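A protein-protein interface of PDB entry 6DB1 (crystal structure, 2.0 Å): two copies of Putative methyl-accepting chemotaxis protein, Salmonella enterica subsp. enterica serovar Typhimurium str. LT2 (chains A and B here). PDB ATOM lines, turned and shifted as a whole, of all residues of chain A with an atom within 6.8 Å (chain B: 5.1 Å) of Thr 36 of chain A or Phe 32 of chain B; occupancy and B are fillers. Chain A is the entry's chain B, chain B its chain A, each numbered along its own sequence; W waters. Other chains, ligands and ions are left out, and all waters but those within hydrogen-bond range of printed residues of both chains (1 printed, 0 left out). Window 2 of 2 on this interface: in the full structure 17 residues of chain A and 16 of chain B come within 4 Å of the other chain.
Phe 32 of chain B touches its own counterpart, Phe 32 of chain A.
Thr 36 of chain A touches Phe 32 of chain B, but with the chains exchanged Phe 32 of chain A does not touch Thr 36 of chain B (10.6 Å).
Water W1 lies within hydrogen-bond range of the backbone carbonyl oxygen (O) of Gly 129 of chain B, the guanidinium group (NE) of Arg 33 of chain A and the side-chain carboxylate (OE2) of Glu 133 of chain B.
Of the printed residues of chain B, Phe 32 of chain A touches Asn 28 (3.95 Å), Asp 29 (3.4 Å) and Phe 32 (3.7 Å).
Printed residues of chain B within 4 Å of Arg 33 of chain A: Asn 28 and Glu 133.
Of chain B, only Phe 32 (3.7 Å) comes within 4 Å of Thr 36 of chain A.
Of the printed residues of chain A, Asn 28 of chain B touches Phe 32 and Arg 33.
Printed residues of chain A within 4 Å of Glu 133 of chain B: Arg 33 (3.8 Å) and Arg 37 (3.2 Å).
The nearest printed residue of chain A that does not touch Asp 29 of chain B is Tyr 31 of chain A (6.0 Å).
The guanidinium group (NH1) of Arg 33 of chain A sits close to the side-chain amide nitrogen (ND2) of Asn 28 of chain B, 3.3 Å away.
The side-chain carboxylate (OE2) of Glu 133 of chain B lies within salt-bridge range of the guanidinium group (NE) of Arg 33 of chain A (3.9 Å).
The guanidinium group (NH2) of Arg 37 of chain A lies within salt-bridge range of the side-chain carboxylate (OE1) of Glu 133 of chain B, 3.2 Å away.
NE of Arg 33 of chain B lies within salt-bridge range of OD2 of Asp 29 of chain B.
The backbone carbonyl oxygen (O) of Phe 32 of chain A sits at hydrogen-bond distance from the side-chain hydroxyl (OG1) of Thr 36 of chain A, at 2.8 Å.
Of the 11 printed residues of chain B, 4 touch a printed residue of chain A.
Hydrophobic or aromatic side chains of chain B within 4 Å of the printed part of chain A: Phe 32.
Among the printed residues, Asp or Glu carboxylates within 4 Å of a Lys or Arg side-chain nitrogen of the other chain: Arg 33 of chain A with Glu 133 of chain B (3.9 Å) and Arg 37 of chain A with Glu 133 of chain B (3.2 Å).
Asn 28 of chain B touches Phe 32 of chain A.
Phe 32 of chain A touches Asp 29 of chain B (CZ to CB, 3.4 Å).
Phe 32 of chain B touches Phe 32 of chain A (CE2 to CD1, 3.7 Å).
Thr 36 of chain A touches Phe 32 of chain B (OG1 to CZ, 3.7 Å).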
ATOM      1  N   TYR A  31      -8.906  20.166  24.232  1.00  0.00           N
ATOM      2  CA  TYR A  31      -8.695  20.243  22.831  1.00  0.00           C
ATOM      3  C   TYR A  31      -9.673  21.258  22.237  1.00  0.00           C
ATOM      4  O   TYR A  31      -9.265  22.176  21.527  1.00  0.00           O
ATOM      5  CB  TYR A  31      -8.859  18.875  22.174  1.00  0.00           C
ATOM      6  CG  TYR A  31      -8.948  18.958  20.677  1.00  0.00           C
ATOM      7  CD1 TYR A  31      -7.831  19.269  19.913  1.00  0.00           C
ATOM      8  CD2 TYR A  31     -10.151  18.780  20.023  1.00  0.00           C
ATOM      9  CE1 TYR A  31      -7.901  19.366  18.534  1.00  0.00           C
ATOM     10  CE2 TYR A  31     -10.242  18.894  18.645  1.00  0.00           C
ATOM     11  CZ  TYR A  31      -9.109  19.168  17.899  1.00  0.00           C
ATOM     12  OH  TYR A  31      -9.182  19.294  16.547  1.00  0.00           O
ATOM     13  N   PHE A  32     -10.964  21.093  22.546  1.00  0.00           N
ATOM     14  CA  PHE A  32     -11.970  22.000  22.010  1.00  0.00           C
ATOM     15  C   PHE A  32     -11.728  23.413  22.529  1.00  0.00           C
ATOM     16  O   PHE A  32     -11.939  24.343  21.793  1.00  0.00           O
ATOM     17  CB  PHE A  32     -13.393  21.488  22.272  1.00  0.00           C
ATOM     18  CG  PHE A  32     -13.723  20.278  21.437  1.00  0.00           C
ATOM     19  CD1 PHE A  32     -13.980  20.410  20.081  1.00  0.00           C
ATOM     20  CD2 PHE A  32     -13.710  19.004  21.986  1.00  0.00           C
ATOM     21  CE1 PHE A  32     -14.226  19.298  19.294  1.00  0.00           C
ATOM     22  CE2 PHE A  32     -13.968  17.894  21.200  1.00  0.00           C
ATOM     23  CZ  PHE A  32     -14.214  18.043  19.857  1.00  0.00           C
ATOM     24  N   ARG A  33     -11.299  23.581  23.772  1.00  0.00           N
ATOM     25  CA  ARG A  33     -11.035  24.923  24.275  1.00  0.00           C
ATOM     26  C   ARG A  33      -9.924  25.556  23.419  1.00  0.00           C
ATOM     27  O   ARG A  33     -10.002  26.726  23.047  1.00  0.00           O
ATOM     28  CB  ARG A  33     -10.589  24.915  25.743  1.00  0.00           C
ATOM     29  CG  ARG A  33     -11.568  24.296  26.736  1.00  0.00           C
ATOM     30  CD  ARG A  33     -12.847  25.085  26.977  1.00  0.00           C
ATOM     31  NE  ARG A  33     -13.711  25.183  25.805  1.00  0.00           N
ATOM     32  CZ  ARG A  33     -14.580  24.242  25.425  1.00  0.00           C
ATOM     33  NH1 ARG A  33     -15.317  24.409  24.338  1.00  0.00           N
ATOM     34  NH2 ARG A  33     -14.682  23.128  26.126  1.00  0.00           N
ATOM     35  N   PHE A  34      -8.890  24.761  23.141  1.00  0.00           N
ATOM     36  CA  PHE A  34      -7.725  25.184  22.354  1.00  0.00           C
ATOM     37  C   PHE A  34      -8.130  25.613  20.948  1.00  0.00           C
ATOM     38  O   PHE A  34      -7.752  26.700  20.490  1.00  0.00           O
ATOM     39  CB  PHE A  34      -6.708  24.058  22.191  1.00  0.00           C
ATOM     40  CG  PHE A  34      -5.735  24.285  21.058  1.00  0.00           C
ATOM     41  CD1 PHE A  34      -4.636  25.119  21.219  1.00  0.00           C
ATOM     42  CD2 PHE A  34      -5.915  23.660  19.832  1.00  0.00           C
ATOM     43  CE1 PHE A  34      -3.749  25.322  20.176  1.00  0.00           C
ATOM     44  CE2 PHE A  34      -5.006  23.846  18.801  1.00  0.00           C
ATOM     45  CZ  PHE A  34      -3.943  24.690  18.968  1.00  0.00           C
ATOM     46  N   VAL A  35      -8.857  24.744  20.256  1.00  0.00           N
ATOM     47  CA  VAL A  35      -9.268  25.092  18.895  1.00  0.00           C
ATOM     48  C   VAL A  35     -10.088  26.389  18.938  1.00  0.00           C
ATOM     49  O   VAL A  35      -9.820  27.335  18.190  1.00  0.00           O
ATOM     50  CB  VAL A  35     -10.072  23.960  18.230  1.00  0.00           C
ATOM     51  CG1 VAL A  35     -10.687  24.404  16.917  1.00  0.00           C
ATOM     52  CG2 VAL A  35      -9.238  22.709  18.036  1.00  0.00           C
ATOM     53  N   THR A  36     -11.085  26.439  19.823  1.00  0.00           N
ATOM     54  CA  THR A  36     -11.959  27.628  19.897  1.00  0.00           C
ATOM     55  C   THR A  36     -11.175  28.917  20.230  1.00  0.00           C
ATOM     56  O   THR A  36     -11.448  29.979  19.666  1.00  0.00           O
ATOM     57  CB  THR A  36     -13.073  27.439  20.930  1.00  0.00           C
ATOM     58  OG1 THR A  36     -13.740  26.213  20.628  1.00  0.00           O
ATOM     59  CG2 THR A  36     -14.058  28.589  20.934  1.00  0.00           C
ATOM     60  N   ARG A  37     -10.230  28.842  21.155  1.00  0.00           N
ATOM     61  CA  ARG A  37      -9.497  30.024  21.556  1.00  0.00           C
ATOM     62  C   ARG A  37      -8.511  30.441  20.447  1.00  0.00           C
ATOM     63  O   ARG A  37      -8.310  31.667  20.188  1.00  0.00           O
ATOM     64  CB  ARG A  37      -8.771  29.748  22.876  1.00  0.00           C
ATOM     65  CG  ARG A  37      -9.656  29.562  24.104  1.00  0.00           C
ATOM     66  CD  ARG A  37      -8.763  29.204  25.277  1.00  0.00           C
ATOM     67  NE  ARG A  37      -9.407  29.251  26.578  1.00  0.00           N
ATOM     68  CZ  ARG A  37      -8.750  29.226  27.733  1.00  0.00           C
ATOM     69  NH1 ARG A  37      -7.429  29.158  27.738  1.00  0.00           N
ATOM     70  NH2 ARG A  37      -9.407  29.325  28.878  1.00  0.00           N
ATOM     71  N   LEU A  38      -7.892  29.455  19.782  1.00  0.00           N
ATOM     72  CA  LEU A  38      -6.927  29.786  18.743  1.00  0.00           C
ATOM     73  C   LEU A  38      -7.665  30.419  17.568  1.00  0.00           C
ATOM     74  O   LEU A  38      -7.136  31.295  16.896  1.00  0.00           O
ATOM     75  CB  LEU A  38      -6.157  28.544  18.282  1.00  0.00           C
ATOM     76  CG  LEU A  38      -5.090  28.810  17.222  1.00  0.00           C
ATOM     77  CD1 LEU A  38      -4.059  29.809  17.731  1.00  0.00           C
ATOM     78  CD2 LEU A  38      -4.404  27.527  16.790  1.00  0.00           C
ATOM     79  N   SER A  39      -8.870  29.944  17.330  1.00  0.00           N
ATOM     80  CA  SER A  39      -9.671  30.460  16.238  1.00  0.00           C
ATOM     81  C   SER A  39     -10.009  31.939  16.500  1.00  0.00           C
ATOM     82  O   SER A  39      -9.813  32.798  15.625  1.00  0.00           O
ATOM     83  CB  SER A  39     -10.888  29.611  16.052  1.00  0.00           C
ATOM     84  OG  SER A  39     -11.579  29.963  14.871  1.00  0.00           O
ATOM     85  N   ARG A  40     -10.446  32.242  17.724  1.00  0.00           N
ATOM     86  CA  ARG A  40     -10.788  33.609  18.137  1.00  0.00           C
ATOM     87  C   ARG A  40      -9.602  34.538  17.827  1.00  0.00           C
ATOM     88  O   ARG A  40      -9.706  35.490  17.039  1.00  0.00           O
ATOM     89  CB  ARG A  40     -11.071  33.662  19.644  1.00  0.00           C
ATOM     90  CG  ARG A  40     -11.855  34.887  20.103  1.00  0.00           C
ATOM     91  CD  ARG A  40     -11.497  35.389  21.502  1.00  0.00           C
ATOM     92  NE  ARG A  40     -11.139  34.352  22.475  1.00  0.00           N
ATOM     93  CZ  ARG A  40     -10.803  34.583  23.748  1.00  0.00           C
ATOM     94  NH1 ARG A  40     -10.387  33.582  24.512  1.00  0.00           N
ATOM     95  NH2 ARG A  40     -10.865  35.812  24.240  1.00  0.00           N
ATOM     96  N   ALA A  41      -8.463  34.223  18.448  1.00  0.00           N
ATOM     97  CA  ALA A  41      -7.234  34.980  18.289  1.00  0.00           C
ATOM     98  C   ALA A  41      -6.874  35.098  16.805  1.00  0.00           C
ATOM     99  O   ALA A  41      -6.391  36.154  16.370  1.00  0.00           O
ATOM    100  CB  ALA A  41      -6.112  34.327  19.058  1.00  0.00           C
ATOM    101  N   ASN B  28     -19.891  19.701  20.429  1.00  0.00           N
ATOM    102  CA  ASN B  28     -18.959  20.684  19.849  1.00  0.00           C
ATOM    103  C   ASN B  28     -18.275  20.078  18.617  1.00  0.00           C
ATOM    104  O   ASN B  28     -18.124  20.722  17.575  1.00  0.00           O
ATOM    105  CB  ASN B  28     -17.947  21.105  20.911  1.00  0.00           C
ATOM    106  CG  ASN B  28     -17.396  22.495  20.710  1.00  0.00           C
ATOM    107  OD1 ASN B  28     -17.376  23.014  19.599  1.00  0.00           O
ATOM    108  ND2 ASN B  28     -16.967  23.112  21.794  1.00  0.00           N
ATOM    109  N   ASP B  29     -17.811  18.844  18.770  1.00  0.00           N
ATOM    110  CA  ASP B  29     -17.205  18.150  17.685  1.00  0.00           C
ATOM    111  C   ASP B  29     -18.184  18.043  16.492  1.00  0.00           C
ATOM    112  O   ASP B  29     -17.795  18.291  15.356  1.00  0.00           O
ATOM    113  CB  ASP B  29     -16.806  16.753  18.114  1.00  0.00           C
ATOM    114  CG  ASP B  29     -16.118  16.001  17.024  1.00  0.00           C
ATOM    115  OD1 ASP B  29     -15.259  16.579  16.312  1.00  0.00           O
ATOM    116  OD2 ASP B  29     -16.440  14.819  16.883  1.00  0.00           O
ATOM    117  N   GLN B  30     -19.444  17.704  16.772  1.00  0.00           N
ATOM    118  CA  GLN B  30     -20.470  17.524  15.716  1.00  0.00           C
ATOM    119  C   GLN B  30     -20.822  18.861  15.051  1.00  0.00           C
ATOM    120  O   GLN B  30     -21.193  18.899  13.860  1.00  0.00           O
ATOM    121  CB  GLN B  30     -21.726  16.863  16.273  1.00  0.00           C
ATOM    122  CG  GLN B  30     -21.490  15.443  16.766  1.00  0.00           C
ATOM    123  CD  GLN B  30     -21.095  14.513  15.651  1.00  0.00           C
ATOM    124  OE1 GLN B  30     -21.553  14.633  14.519  1.00  0.00           O
ATOM    125  NE2 GLN B  30     -20.260  13.550  15.984  1.00  0.00           N
ATOM    126  N   TYR B  31     -20.748  19.940  15.815  1.00  0.00           N
ATOM    127  CA  TYR B  31     -20.972  21.225  15.240  1.00  0.00           C
ATOM    128  C   TYR B  31     -19.799  21.577  14.307  1.00  0.00           C
ATOM    129  O   TYR B  31     -20.026  21.967  13.148  1.00  0.00           O
ATOM    130  CB  TYR B  31     -21.164  22.280  16.326  1.00  0.00           C
ATOM    131  CG  TYR B  31     -21.036  23.683  15.797  1.00  0.00           C
ATOM    132  CD1 TYR B  31     -22.001  24.218  14.959  1.00  0.00           C
ATOM    133  CD2 TYR B  31     -19.926  24.455  16.100  1.00  0.00           C
ATOM    134  CE1 TYR B  31     -21.869  25.494  14.441  1.00  0.00           C
ATOM    135  CE2 TYR B  31     -19.786  25.738  15.596  1.00  0.00           C
ATOM    136  CZ  TYR B  31     -20.762  26.258  14.765  1.00  0.00           C
ATOM    137  OH  TYR B  31     -20.637  27.525  14.273  1.00  0.00           O
ATOM    138  N   PHE B  32     -18.549  21.433  14.772  1.00  0.00           N
ATOM    139  CA  PHE B  32     -17.421  21.773  13.901  1.00  0.00           C
ATOM    140  C   PHE B  32     -17.479  20.904  12.649  1.00  0.00           C
ATOM    141  O   PHE B  32     -17.229  21.398  11.550  1.00  0.00           O
ATOM    142  CB  PHE B  32     -16.052  21.661  14.581  1.00  0.00           C
ATOM    143  CG  PHE B  32     -15.817  22.648  15.698  1.00  0.00           C
ATOM    144  CD1 PHE B  32     -16.321  23.938  15.628  1.00  0.00           C
ATOM    145  CD2 PHE B  32     -14.984  22.331  16.756  1.00  0.00           C
ATOM    146  CE1 PHE B  32     -16.087  24.853  16.643  1.00  0.00           C
ATOM    147  CE2 PHE B  32     -14.741  23.251  17.767  1.00  0.00           C
ATOM    148  CZ  PHE B  32     -15.295  24.510  17.712  1.00  0.00           C
ATOM    149  N   ARG B  33     -17.826  19.636  12.809  1.00  0.00           N
ATOM    150  CA  ARG B  33     -17.917  18.782  11.658  1.00  0.00           C
ATOM    151  C   ARG B  33     -18.935  19.365  10.680  1.00  0.00           C
ATOM    152  O   ARG B  33     -18.621  19.562   9.514  1.00  0.00           O
ATOM    153  CB  ARG B  33     -18.291  17.347  12.035  1.00  0.00           C
ATOM    154  CG  ARG B  33     -17.140  16.537  12.616  1.00  0.00           C
ATOM    155  CD  ARG B  33     -17.579  15.130  12.962  1.00  0.00           C
ATOM    156  NE  ARG B  33     -16.453  14.306  13.351  1.00  0.00           N
ATOM    157  CZ  ARG B  33     -16.549  13.034  13.709  1.00  0.00           C
ATOM    158  NH1 ARG B  33     -17.737  12.455  13.755  1.00  0.00           N
ATOM    159  NH2 ARG B  33     -15.459  12.349  14.012  1.00  0.00           N
ATOM    160  N   PHE B  34     -20.127  19.655  11.176  1.00  0.00           N
ATOM    161  CA  PHE B  34     -21.201  20.176  10.365  1.00  0.00           C
ATOM    162  C   PHE B  34     -20.723  21.305   9.450  1.00  0.00           C
ATOM    163  O   PHE B  34     -21.079  21.324   8.287  1.00  0.00           O
ATOM    164  CB  PHE B  34     -22.337  20.707  11.238  1.00  0.00           C
ATOM    165  CG  PHE B  34     -23.323  21.544  10.470  1.00  0.00           C
ATOM    166  CD1 PHE B  34     -24.305  20.946   9.700  1.00  0.00           C
ATOM    167  CD2 PHE B  34     -23.244  22.926  10.491  1.00  0.00           C
ATOM    168  CE1 PHE B  34     -25.194  21.712   8.968  1.00  0.00           C
ATOM    169  CE2 PHE B  34     -24.141  23.691   9.764  1.00  0.00           C
ATOM    170  CZ  PHE B  34     -25.107  23.083   8.997  1.00  0.00           C
ATOM    171  N   VAL B  35     -19.944  22.236   9.990  1.00  0.00           N
ATOM    172  CA  VAL B  35     -19.483  23.386   9.243  1.00  0.00           C
ATOM    173  C   VAL B  35     -18.573  22.940   8.097  1.00  0.00           C
ATOM    174  O   VAL B  35     -18.620  23.523   7.029  1.00  0.00           O
ATOM    175  CB  VAL B  35     -18.761  24.398  10.150  1.00  0.00           C
ATOM    176  CG1 VAL B  35     -18.100  25.505   9.340  1.00  0.00           C
ATOM    177  CG2 VAL B  35     -19.699  24.984  11.193  1.00  0.00           C
ATOM    178  N   THR B  36     -17.746  21.923   8.325  1.00  0.00           N
ATOM    179  CA  THR B  36     -16.830  21.456   7.294  1.00  0.00           C
ATOM    180  C   THR B  36     -17.573  20.588   6.273  1.00  0.00           C
ATOM    181  O   THR B  36     -17.399  20.755   5.060  1.00  0.00           O
ATOM    182  CB  THR B  36     -15.651  20.680   7.889  1.00  0.00           C
ATOM    183  OG1 THR B  36     -16.142  19.463   8.449  1.00  0.00           O
ATOM    184  CG2 THR B  36     -14.898  21.462   8.942  1.00  0.00           C
ATOM    185  N   GLY B 129     -19.454  28.875  22.587  1.00  0.00           N
ATOM    186  CA  GLY B 129     -18.087  28.661  23.056  1.00  0.00           C
ATOM    187  C   GLY B 129     -17.857  29.281  24.424  1.00  0.00           C
ATOM    188  O   GLY B 129     -17.114  28.719  25.241  1.00  0.00           O
ATOM    189  N   GLU B 133     -16.967  27.190  27.828  1.00  0.00           N
ATOM    190  CA  GLU B 133     -15.802  27.537  28.660  1.00  0.00           C
ATOM    191  C   GLU B 133     -16.222  27.649  30.125  1.00  0.00           C
ATOM    192  O   GLU B 133     -15.535  27.176  31.021  1.00  0.00           O
ATOM    193  CB  GLU B 133     -15.190  28.877  28.237  1.00  0.00           C
ATOM    194  CG  GLU B 133     -14.553  28.862  26.858  1.00  0.00           C
ATOM    195  CD  GLU B 133     -13.033  28.918  26.817  1.00  0.00           C
ATOM    196  OE1 GLU B 133     -12.416  28.948  27.893  1.00  0.00           O
ATOM    197  OE2 GLU B 133     -12.476  28.901  25.696  1.00  0.00           O
HETATM  198  O   HOH W   1     -14.794  27.397  24.147  1.00  0.00           O
